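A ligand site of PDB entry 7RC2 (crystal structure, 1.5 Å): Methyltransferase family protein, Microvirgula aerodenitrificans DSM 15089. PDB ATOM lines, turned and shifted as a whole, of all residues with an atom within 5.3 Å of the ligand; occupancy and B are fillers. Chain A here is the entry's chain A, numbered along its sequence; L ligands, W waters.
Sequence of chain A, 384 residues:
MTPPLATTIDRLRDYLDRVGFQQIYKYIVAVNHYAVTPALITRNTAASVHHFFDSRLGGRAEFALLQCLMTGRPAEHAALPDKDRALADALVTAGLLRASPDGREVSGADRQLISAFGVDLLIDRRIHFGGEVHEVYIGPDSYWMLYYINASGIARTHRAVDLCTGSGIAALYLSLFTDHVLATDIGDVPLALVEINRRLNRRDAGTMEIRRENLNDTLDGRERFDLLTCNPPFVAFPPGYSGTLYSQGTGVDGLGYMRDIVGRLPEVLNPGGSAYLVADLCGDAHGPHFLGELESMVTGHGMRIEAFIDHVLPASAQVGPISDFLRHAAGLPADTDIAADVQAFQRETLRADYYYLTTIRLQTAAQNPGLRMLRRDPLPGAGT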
ATOM      1  N   TYR A 137      21.650  -9.719  21.523  1.00  0.00           N
ATOM      2  CA  TYR A 137      22.021  -8.429  20.960  1.00  0.00           C
ATOM      3  C   TYR A 137      22.275  -8.530  19.468  1.00  0.00           C
ATOM      4  O   TYR A 137      22.853  -9.505  18.989  1.00  0.00           O
ATOM      5  CB  TYR A 137      23.303  -7.901  21.640  1.00  0.00           C
ATOM      6  CG  TYR A 137      23.672  -6.567  21.064  1.00  0.00           C
ATOM      7  CD1 TYR A 137      23.058  -5.410  21.516  1.00  0.00           C
ATOM      8  CD2 TYR A 137      24.588  -6.458  20.009  1.00  0.00           C
ATOM      9  CE1 TYR A 137      23.345  -4.183  20.956  1.00  0.00           C
ATOM     10  CE2 TYR A 137      24.875  -5.231  19.449  1.00  0.00           C
ATOM     11  CZ  TYR A 137      24.236  -4.101  19.928  1.00  0.00           C
ATOM     12  OH  TYR A 137      24.506  -2.873  19.391  1.00  0.00           O
ATOM     13  N   ILE A 138      21.866  -7.486  18.744  1.00  0.00           N
ATOM     14  CA  ILE A 138      22.414  -7.150  17.424  1.00  0.00           C
ATOM     15  C   ILE A 138      22.223  -5.645  17.237  1.00  0.00           C
ATOM     16  O   ILE A 138      21.303  -5.056  17.804  1.00  0.00           O
ATOM     17  CB  ILE A 138      21.765  -7.979  16.286  1.00  0.00           C
ATOM     18  CG1 ILE A 138      22.620  -7.899  15.022  1.00  0.00           C
ATOM     19  CG2 ILE A 138      20.342  -7.504  15.983  1.00  0.00           C
ATOM     20  CD1 ILE A 138      22.112  -8.801  13.894  1.00  0.00           C
ATOM     21  N   GLY A 139      23.119  -5.016  16.472  1.00  0.00           N
ATOM     22  CA  GLY A 139      23.042  -3.573  16.301  1.00  0.00           C
ATOM     23  C   GLY A 139      23.891  -3.067  15.149  1.00  0.00           C
ATOM     24  O   GLY A 139      24.547  -3.835  14.453  1.00  0.00           O
ATOM     25  N   SER A 142      27.426  -4.249  15.088  1.00  0.00           N
ATOM     26  CA  SER A 142      27.589  -5.573  14.508  1.00  0.00           C
ATOM     27  C   SER A 142      27.853  -5.477  13.013  1.00  0.00           C
ATOM     28  O   SER A 142      28.740  -6.151  12.471  1.00  0.00           O
ATOM     29  CB  SER A 142      26.328  -6.410  14.756  1.00  0.00           C
ATOM     30  OG  SER A 142      25.826  -6.248  16.089  1.00  0.00           O
ATOM     31  N   MET A 145      31.427  -3.668  12.001  1.00  0.00           N
ATOM     32  CA  MET A 145      32.511  -4.636  12.153  1.00  0.00           C
ATOM     33  C   MET A 145      32.709  -5.436  10.870  1.00  0.00           C
ATOM     34  O   MET A 145      33.838  -5.629  10.399  1.00  0.00           O
ATOM     35  CB  MET A 145      32.184  -5.611  13.283  1.00  0.00           C
ATOM     36  CG  MET A 145      33.297  -6.624  13.539  1.00  0.00           C
ATOM     37  SD  MET A 145      33.087  -7.499  15.099  1.00  0.00           S
ATOM     38  CE  MET A 145      31.757  -8.531  14.544  1.00  0.00           C
ATOM     39  N   ASP A 162      34.764 -16.259  15.221  1.00  0.00           N
ATOM     40  CA  ASP A 162      33.883 -15.185  15.684  1.00  0.00           C
ATOM     41  C   ASP A 162      33.640 -15.424  17.176  1.00  0.00           C
ATOM     42  O   ASP A 162      32.838 -16.288  17.541  1.00  0.00           O
ATOM     43  CB  ASP A 162      32.580 -15.181  14.890  1.00  0.00           C
ATOM     44  CG  ASP A 162      31.631 -14.094  15.337  1.00  0.00           C
ATOM     45  OD1 ASP A 162      32.114 -13.002  15.682  1.00  0.00           O
ATOM     46  OD2 ASP A 162      30.402 -14.344  15.312  1.00  0.00           O
ATOM     47  N   LEU A 163      34.340 -14.652  18.013  1.00  0.00           N
ATOM     48  CA  LEU A 163      34.134 -14.714  19.453  1.00  0.00           C
ATOM     49  C   LEU A 163      32.897 -13.918  19.855  1.00  0.00           C
ATOM     50  O   LEU A 163      32.665 -12.822  19.344  1.00  0.00           O
ATOM     51  CB  LEU A 163      35.348 -14.146  20.194  1.00  0.00           C
ATOM     52  CG  LEU A 163      36.687 -14.806  19.885  1.00  0.00           C
ATOM     53  CD1 LEU A 163      37.821 -13.931  20.420  1.00  0.00           C
ATOM     54  CD2 LEU A 163      36.747 -16.202  20.497  1.00  0.00           C
ATOM     55  N   CYS A 164      32.117 -14.467  20.788  1.00  0.00           N
ATOM     56  CA  CYS A 164      30.938 -13.759  21.325  1.00  0.00           C
ATOM     57  C   CYS A 164      29.909 -13.562  20.221  1.00  0.00           C
ATOM     58  O   CYS A 164      29.478 -12.442  19.923  1.00  0.00           O
ATOM     59  CB  CYS A 164      31.310 -12.404  21.943  1.00  0.00           C
ATOM     60  SG  CYS A 164      32.637 -12.386  23.157  1.00  0.00           S
ATOM     61  N   THR A 165      29.502 -14.687  19.617  1.00  0.00           N
ATOM     62  CA  THR A 165      28.799 -14.683  18.341  1.00  0.00           C
ATOM     63  C   THR A 165      27.356 -14.170  18.415  1.00  0.00           C
ATOM     64  O   THR A 165      26.825 -13.676  17.413  1.00  0.00           O
ATOM     65  CB  THR A 165      28.867 -16.093  17.732  1.00  0.00           C
ATOM     66  OG1 THR A 165      28.590 -16.032  16.326  1.00  0.00           O
ATOM     67  CG2 THR A 165      27.901 -17.040  18.411  1.00  0.00           C
ATOM     68  N   GLY A 166      26.696 -14.279  19.561  1.00  0.00           N
ATOM     69  CA  GLY A 166      25.329 -13.755  19.638  1.00  0.00           C
ATOM     70  C   GLY A 166      24.394 -14.507  18.699  1.00  0.00           C
ATOM     71  O   GLY A 166      24.268 -15.733  18.762  1.00  0.00           O
ATOM     72  N   SER A 167      23.739 -13.754  17.801  1.00  0.00           N
ATOM     73  CA  SER A 167      22.856 -14.342  16.794  1.00  0.00           C
ATOM     74  C   SER A 167      23.609 -15.215  15.797  1.00  0.00           C
ATOM     75  O   SER A 167      22.981 -16.043  15.113  1.00  0.00           O
ATOM     76  CB  SER A 167      22.138 -13.225  16.033  1.00  0.00           C
ATOM     77  OG  SER A 167      23.051 -12.507  15.196  1.00  0.00           O
ATOM     78  N   ILE A 169      25.661 -13.685  13.426  1.00  0.00           N
ATOM     79  CA  ILE A 169      25.766 -12.920  12.180  1.00  0.00           C
ATOM     80  C   ILE A 169      27.200 -12.906  11.641  1.00  0.00           C
ATOM     81  O   ILE A 169      27.426 -13.161  10.461  1.00  0.00           O
ATOM     82  CB  ILE A 169      25.208 -11.495  12.360  1.00  0.00           C
ATOM     83  CG1 ILE A 169      25.384 -10.704  11.051  1.00  0.00           C
ATOM     84  CG2 ILE A 169      25.824 -10.771  13.533  1.00  0.00           C
ATOM     85  CD1 ILE A 169      24.861  -9.298  11.126  1.00  0.00           C
ATOM     86  N   ALA A 170      28.187 -12.594  12.484  1.00  0.00           N
ATOM     87  CA  ALA A 170      29.553 -12.474  11.959  1.00  0.00           C
ATOM     88  C   ALA A 170      30.091 -13.829  11.515  1.00  0.00           C
ATOM     89  O   ALA A 170      30.710 -13.948  10.449  1.00  0.00           O
ATOM     90  CB  ALA A 170      30.482 -11.848  12.989  1.00  0.00           C
ATOM     91  N   THR A 184      31.717 -18.753  19.032  1.00  0.00           N
ATOM     92  CA  THR A 184      31.645 -19.028  20.467  1.00  0.00           C
ATOM     93  C   THR A 184      30.675 -18.105  21.197  1.00  0.00           C
ATOM     94  O   THR A 184      30.466 -16.954  20.815  1.00  0.00           O
ATOM     95  CB  THR A 184      33.020 -18.896  21.140  1.00  0.00           C
ATOM     96  OG1 THR A 184      33.359 -17.501  21.249  1.00  0.00           O
ATOM     97  CG2 THR A 184      34.110 -19.639  20.365  1.00  0.00           C
ATOM     98  N   ASP A 185      30.118 -18.608  22.300  1.00  0.00           N
ATOM     99  CA  ASP A 185      29.338 -17.763  23.200  1.00  0.00           C
ATOM    100  C   ASP A 185      29.205 -18.528  24.504  1.00  0.00           C
ATOM    101  O   ASP A 185      29.608 -19.691  24.599  1.00  0.00           O
ATOM    102  CB  ASP A 185      27.963 -17.406  22.605  1.00  0.00           C
ATOM    103  CG  ASP A 185      27.432 -16.065  23.090  1.00  0.00           C
ATOM    104  OD1 ASP A 185      27.170 -15.906  24.301  1.00  0.00           O
ATOM    105  OD2 ASP A 185      27.257 -15.150  22.254  1.00  0.00           O
ATOM    106  N   ILE A 186      28.632 -17.878  25.522  1.00  0.00           N
ATOM    107  CA  ILE A 186      28.370 -18.563  26.788  1.00  0.00           C
ATOM    108  C   ILE A 186      26.924 -18.436  27.241  1.00  0.00           C
ATOM    109  O   ILE A 186      26.525 -19.045  28.246  1.00  0.00           O
ATOM    110  CB  ILE A 186      29.302 -18.077  27.916  1.00  0.00           C
ATOM    111  CG1 ILE A 186      29.163 -16.572  28.170  1.00  0.00           C
ATOM    112  CG2 ILE A 186      30.756 -18.457  27.587  1.00  0.00           C
ATOM    113  CD1 ILE A 186      29.961 -16.096  29.366  1.00  0.00           C
ATOM    114  N   GLY A 187      26.113 -17.645  26.535  1.00  0.00           N
ATOM    115  CA  GLY A 187      24.706 -17.482  26.910  1.00  0.00           C
ATOM    116  C   GLY A 187      23.845 -18.573  26.297  1.00  0.00           C
ATOM    117  O   GLY A 187      23.973 -18.888  25.119  1.00  0.00           O
ATOM    118  N   PRO A 190      21.603 -16.941  23.193  1.00  0.00           N
ATOM    119  CA  PRO A 190      22.300 -16.800  21.915  1.00  0.00           C
ATOM    120  C   PRO A 190      22.813 -18.122  21.363  1.00  0.00           C
ATOM    121  O   PRO A 190      22.753 -18.329  20.148  1.00  0.00           O
ATOM    122  CB  PRO A 190      23.450 -15.815  22.219  1.00  0.00           C
ATOM    123  CG  PRO A 190      23.597 -15.836  23.712  1.00  0.00           C
ATOM    124  CD  PRO A 190      22.192 -16.072  24.233  1.00  0.00           C
ATOM    125  N   GLU A 213      32.008 -21.508  25.182  1.00  0.00           N
ATOM    126  CA  GLU A 213      33.350 -21.281  25.703  1.00  0.00           C
ATOM    127  C   GLU A 213      33.556 -19.808  26.026  1.00  0.00           C
ATOM    128  O   GLU A 213      33.217 -18.949  25.205  1.00  0.00           O
ATOM    129  CB  GLU A 213      34.404 -21.755  24.693  1.00  0.00           C
ATOM    130  CG  GLU A 213      35.838 -21.712  25.195  1.00  0.00           C
ATOM    131  CD  GLU A 213      36.750 -22.528  24.319  1.00  0.00           C
ATOM    132  OE1 GLU A 213      37.174 -22.038  23.252  1.00  0.00           O
ATOM    133  OE2 GLU A 213      37.029 -23.699  24.675  1.00  0.00           O
ATOM    134  N   ASN A 214      34.092 -19.534  27.218  1.00  0.00           N
ATOM    135  CA  ASN A 214      34.475 -18.171  27.615  1.00  0.00           C
ATOM    136  C   ASN A 214      35.522 -17.627  26.649  1.00  0.00           C
ATOM    137  O   ASN A 214      36.440 -18.352  26.247  1.00  0.00           O
ATOM    138  CB  ASN A 214      35.064 -18.139  29.025  1.00  0.00           C
ATOM    139  CG  ASN A 214      34.115 -18.637  30.086  1.00  0.00           C
ATOM    140  OD1 ASN A 214      32.941 -18.259  30.119  1.00  0.00           O
ATOM    141  ND2 ASN A 214      34.634 -19.452  31.001  1.00  0.00           N
ATOM    142  N   LEU A 215      35.427 -16.334  26.333  1.00  0.00           N
ATOM    143  CA  LEU A 215      36.361 -15.811  25.338  1.00  0.00           C
ATOM    144  C   LEU A 215      37.804 -15.904  25.811  1.00  0.00           C
ATOM    145  O   LEU A 215      38.692 -16.183  25.011  1.00  0.00           O
ATOM    146  CB  LEU A 215      36.016 -14.381  24.938  1.00  0.00           C
ATOM    147  CG  LEU A 215      36.198 -13.186  25.855  1.00  0.00           C
ATOM    148  CD1 LEU A 215      37.604 -12.641  25.713  1.00  0.00           C
ATOM    149  CD2 LEU A 215      35.181 -12.100  25.499  1.00  0.00           C
ATOM    150  N   ASN A 231      32.710  -8.635  18.568  1.00  0.00           N
ATOM    151  CA  ASN A 231      31.956  -7.538  19.149  1.00  0.00           C
ATOM    152  C   ASN A 231      31.655  -7.953  20.590  1.00  0.00           C
ATOM    153  O   ASN A 231      30.619  -8.575  20.859  1.00  0.00           O
ATOM    154  CB  ASN A 231      30.680  -7.300  18.352  1.00  0.00           C
ATOM    155  CG  ASN A 231      29.821  -6.190  18.909  1.00  0.00           C
ATOM    156  OD1 ASN A 231      30.161  -5.546  19.910  1.00  0.00           O
ATOM    157  ND2 ASN A 231      28.687  -5.943  18.259  1.00  0.00           N
ATOM    158  N   PRO A 232      32.549  -7.673  21.535  1.00  0.00           N
ATOM    159  CA  PRO A 232      32.362  -8.181  22.908  1.00  0.00           C
ATOM    160  C   PRO A 232      31.457  -7.265  23.695  1.00  0.00           C
ATOM    161  O   PRO A 232      31.197  -6.130  23.267  1.00  0.00           O
ATOM    162  CB  PRO A 232      33.795  -8.145  23.470  1.00  0.00           C
ATOM    163  CG  PRO A 232      34.363  -6.889  22.826  1.00  0.00           C
ATOM    164  CD  PRO A 232      33.781  -6.873  21.401  1.00  0.00           C
ATOM    165  N   PRO A 233      30.974  -7.692  24.856  1.00  0.00           N
ATOM    166  CA  PRO A 233      30.408  -6.721  25.792  1.00  0.00           C
ATOM    167  C   PRO A 233      31.444  -5.645  26.086  1.00  0.00           C
ATOM    168  O   PRO A 233      32.573  -5.957  26.463  1.00  0.00           O
ATOM    169  CB  PRO A 233      30.099  -7.559  27.041  1.00  0.00           C
ATOM    170  CG  PRO A 233      30.027  -8.979  26.558  1.00  0.00           C
ATOM    171  CD  PRO A 233      31.050  -9.040  25.442  1.00  0.00           C
ATOM    172  N   LEU A 245      24.270  -9.833  30.043  1.00  0.00           N
ATOM    173  CA  LEU A 245      25.402 -10.598  29.528  1.00  0.00           C
ATOM    174  C   LEU A 245      25.988  -9.991  28.265  1.00  0.00           C
ATOM    175  O   LEU A 245      27.218  -9.973  28.085  1.00  0.00           O
ATOM    176  CB  LEU A 245      24.958 -12.050  29.283  1.00  0.00           C
ATOM    177  CG  LEU A 245      26.033 -13.010  28.807  1.00  0.00           C
ATOM    178  CD1 LEU A 245      27.151 -13.153  29.833  1.00  0.00           C
ATOM    179  CD2 LEU A 245      25.392 -14.368  28.510  1.00  0.00           C
ATOM    180  N   TYR A 246      25.139  -9.494  27.355  1.00  0.00           N
ATOM    181  CA  TYR A 246      25.646  -8.959  26.101  1.00  0.00           C
ATOM    182  C   TYR A 246      26.182  -7.543  26.212  1.00  0.00           C
ATOM    183  O   TYR A 246      26.959  -7.112  25.354  1.00  0.00           O
ATOM    184  CB  TYR A 246      24.573  -9.004  25.004  1.00  0.00           C
ATOM    185  CG  TYR A 246      23.250  -8.391  25.405  1.00  0.00           C
ATOM    186  CD1 TYR A 246      23.030  -7.015  25.301  1.00  0.00           C
ATOM    187  CD2 TYR A 246      22.211  -9.190  25.883  1.00  0.00           C
ATOM    188  CE1 TYR A 246      21.796  -6.459  25.683  1.00  0.00           C
ATOM    189  CE2 TYR A 246      21.004  -8.646  26.259  1.00  0.00           C
ATOM    190  CZ  TYR A 246      20.799  -7.298  26.158  1.00  0.00           C
ATOM    191  OH  TYR A 246      19.569  -6.779  26.537  1.00  0.00           O
ATOM    192  N   TYR A 257      37.511  -6.880  28.096  1.00  0.00           N
ATOM    193  CA  TYR A 257      37.549  -7.926  27.078  1.00  0.00           C
ATOM    194  C   TYR A 257      38.328  -7.464  25.850  1.00  0.00           C
ATOM    195  O   TYR A 257      38.988  -8.282  25.203  1.00  0.00           O
ATOM    196  CB  TYR A 257      36.118  -8.302  26.675  1.00  0.00           C
ATOM    197  CG  TYR A 257      35.361  -9.144  27.685  1.00  0.00           C
ATOM    198  CD1 TYR A 257      35.975 -10.177  28.383  1.00  0.00           C
ATOM    199  CD2 TYR A 257      34.011  -8.913  27.896  1.00  0.00           C
ATOM    200  CE1 TYR A 257      35.260 -10.955  29.289  1.00  0.00           C
ATOM    201  CE2 TYR A 257      33.287  -9.671  28.803  1.00  0.00           C
ATOM    202  CZ  TYR A 257      33.904 -10.697  29.485  1.00  0.00           C
ATOM    203  OH  TYR A 257      33.156 -11.450  30.357  1.00  0.00           O
HETATM  204  N1  LIG L   1      28.689 -10.879  17.709  1.00  0.00           N
HETATM  205  C1  LIG L   1      27.289 -10.472  17.873  1.00  0.00           C
HETATM  206  C2  LIG L   1      26.903 -10.347  19.346  1.00  0.00           C
HETATM  207  C3  LIG L   1      27.709  -9.334  20.151  1.00  0.00           C
HETATM  208  S1  LIG L   1      26.929  -9.060  21.766  1.00  0.00           S
HETATM  209  C4  LIG L   1      27.058  -9.154  17.141  1.00  0.00           C
HETATM  210  O1  LIG L   1      25.902  -8.764  16.950  1.00  0.00           O
HETATM  211  O2  LIG L   1      28.036  -8.489  16.750  1.00  0.00           O
HETATM  212  C5  LIG L   1      28.160  -9.813  22.865  1.00  0.00           C
HETATM  213  C6  LIG L   1      28.040 -11.331  23.028  1.00  0.00           C
HETATM  214  O3  LIG L   1      29.002 -11.778  23.974  1.00  0.00           O
HETATM  215  C7  LIG L   1      26.696 -11.821  23.581  1.00  0.00           C
HETATM  216  O4  LIG L   1      26.089 -12.735  22.679  1.00  0.00           O
HETATM  217  C8  LIG L   1      27.060 -12.513  24.902  1.00  0.00           C
HETATM  218  O5  LIG L   1      26.294 -13.631  25.254  1.00  0.00           O
HETATM  219  C9  LIG L   1      28.488 -12.928  24.661  1.00  0.00           C
HETATM  220  N2  LIG L   1      29.387 -13.014  25.814  1.00  0.00           N
HETATM  221  C10 LIG L   1      29.390 -12.213  26.929  1.00  0.00           C
HETATM  222  N3  LIG L   1      30.447 -12.565  27.694  1.00  0.00           N
HETATM  223  C11 LIG L   1      31.142 -13.549  27.055  1.00  0.00           C
HETATM  224  C12 LIG L   1      32.297 -14.245  27.377  1.00  0.00           C
HETATM  225  N4  LIG L   1      32.978 -14.011  28.492  1.00  0.00           N
HETATM  226  N5  LIG L   1      32.736 -15.208  26.488  1.00  0.00           N
HETATM  227  C13 LIG L   1      32.053 -15.470  25.319  1.00  0.00           C
HETATM  228  N6  LIG L   1      30.903 -14.777  25.011  1.00  0.00           N
HETATM  229  C14 LIG L   1      30.472 -13.825  25.871  1.00  0.00           C
HETATM  230  O   HOH W   1      23.403 -11.744  22.713  1.00  0.00           O
HETATM  231  O   HOH W   2      28.387 -12.588  15.426  1.00  0.00           O
HETATM  232  O   HOH W   3      30.530 -11.421  30.268  1.00  0.00           O
HETATM  233  O   HOH W   4      27.015  -6.291  22.842  1.00  0.00           O
HETATM  234  O   HOH W   5      24.045 -10.768  17.045  1.00  0.00           O
HETATM  235  O   HOH W   6      23.779 -12.373  25.477  1.00  0.00           O
HETATM  236  O   HOH W   7      31.395 -11.139  17.623  1.00  0.00           O
HETATM  237  O   HOH W   8      36.042 -14.754  29.615  1.00  0.00           O
HETATM  238  O   HOH W   9      28.710  -8.901  13.758  1.00  0.00           O
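Water W5 lies within hydrogen-bond range of O of Tyr 137, OG of Ser 167 and O1 of the ligand. Water W3 lies within hydrogen-bond range of the side-chain hydroxyl of Tyr 257 (2.6 Å) and a nitrogen (N3) of the ligand (2.8 Å). Water W1 bridges an oxygen (O4) of the ligand (2.9 Å) and the backbone NH of Tyr 137 (2.9 Å). Water W2 lies within hydrogen-bond range of OD2 of Asp 162, O of Thr 165, N1 of the ligand and N of Ala 170. Water W4 bridges the backbone carbonyl oxygen of Tyr 246 (2.6 Å) and a sulfur (S1) of the ligand (3.0 Å). Water W9 lies within hydrogen-bond range of the backbone carbonyl oxygen (O) of Ser 142 (3.0 Å) and an oxygen (O2) of the ligand (3.1 Å).
The side-chain hydroxyl (OG) of Ser 167 sits at hydrogen-bond distance from the backbone NH (N) of Ile 169 (3.4 Å). The backbone NH (N) of Asn 231 sits at hydrogen-bond distance from the side-chain sulfur (SD) of Met 145. OD2 of Asp 185 sits at hydrogen-bond distance from N of Gly 166 (2.9 Å). O of Thr 184 sits at hydrogen-bond distance from N of Cys 164 (3.0 Å). The backbone NH (N) of Thr 165 sits at hydrogen-bond distance from the backbone carbonyl oxygen (O) of Thr 184 (2.7 Å). The side-chain hydroxyl (OG) of Ser 142 lies within hydrogen-bond range of the backbone NH (N) of Gly 139, 3.0 Å away. The backbone NH of Gly 187 sits at hydrogen-bond distance from the side-chain carboxylate of Asp 185 (3.0 Å). The backbone carbonyl oxygen (O) of Asp 185 is in hydrogen-bond range of the backbone NH (N) of Glu 213.
The backbone carbonyl oxygen of Cys 164 is in hydrogen-bond range of a nitrogen (N1) of the ligand (2.8 Å). The side-chain hydroxyl (OG) of Ser 142 sits at hydrogen-bond distance from an oxygen (O1) of the ligand (2.7 Å). O of Thr 165 sits close to N1 of the ligand. A nitrogen (N5) of the ligand is in hydrogen-bond range of the backbone NH of Leu 215 (2.9 Å). OH of Tyr 257 is in hydrogen-bond range of N4 of the ligand, at 3.2 Å. The side-chain amide nitrogen (ND2) of Asn 231 sits at hydrogen-bond distance from an oxygen (O2) of the ligand (3.0 Å). N6 of the ligand is in hydrogen-bond range of SG of Cys 164 (3.5 Å). The side-chain carboxylate of Asp 185 sits at hydrogen-bond distance from an oxygen (O5) of the ligand (2.6 Å).
Merely in contact with the ligand: Tyr 137, Ile 138, Gly 166, Ile 169, Ile 186, Pro 190, Glu 213, Asn 214, Pro 233, Leu 245 and Tyr 246. 18 residues have an atom within 4 Å of the ligand: Tyr 137, Ile 138, Ser 142, Cys 164, Thr 165, Gly 166, Ile 169, Asp 185, Ile 186, Pro 190, Glu 213, Asn 214, Leu 215, Asn 231, Pro 233, Leu 245, Tyr 246 and Tyr 257. Along chain A the residues within 4 Å of the ligand span positions 137 to 257. The nearest printed residue that does not touch the ligand is Gly 187 (4.2 Å).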
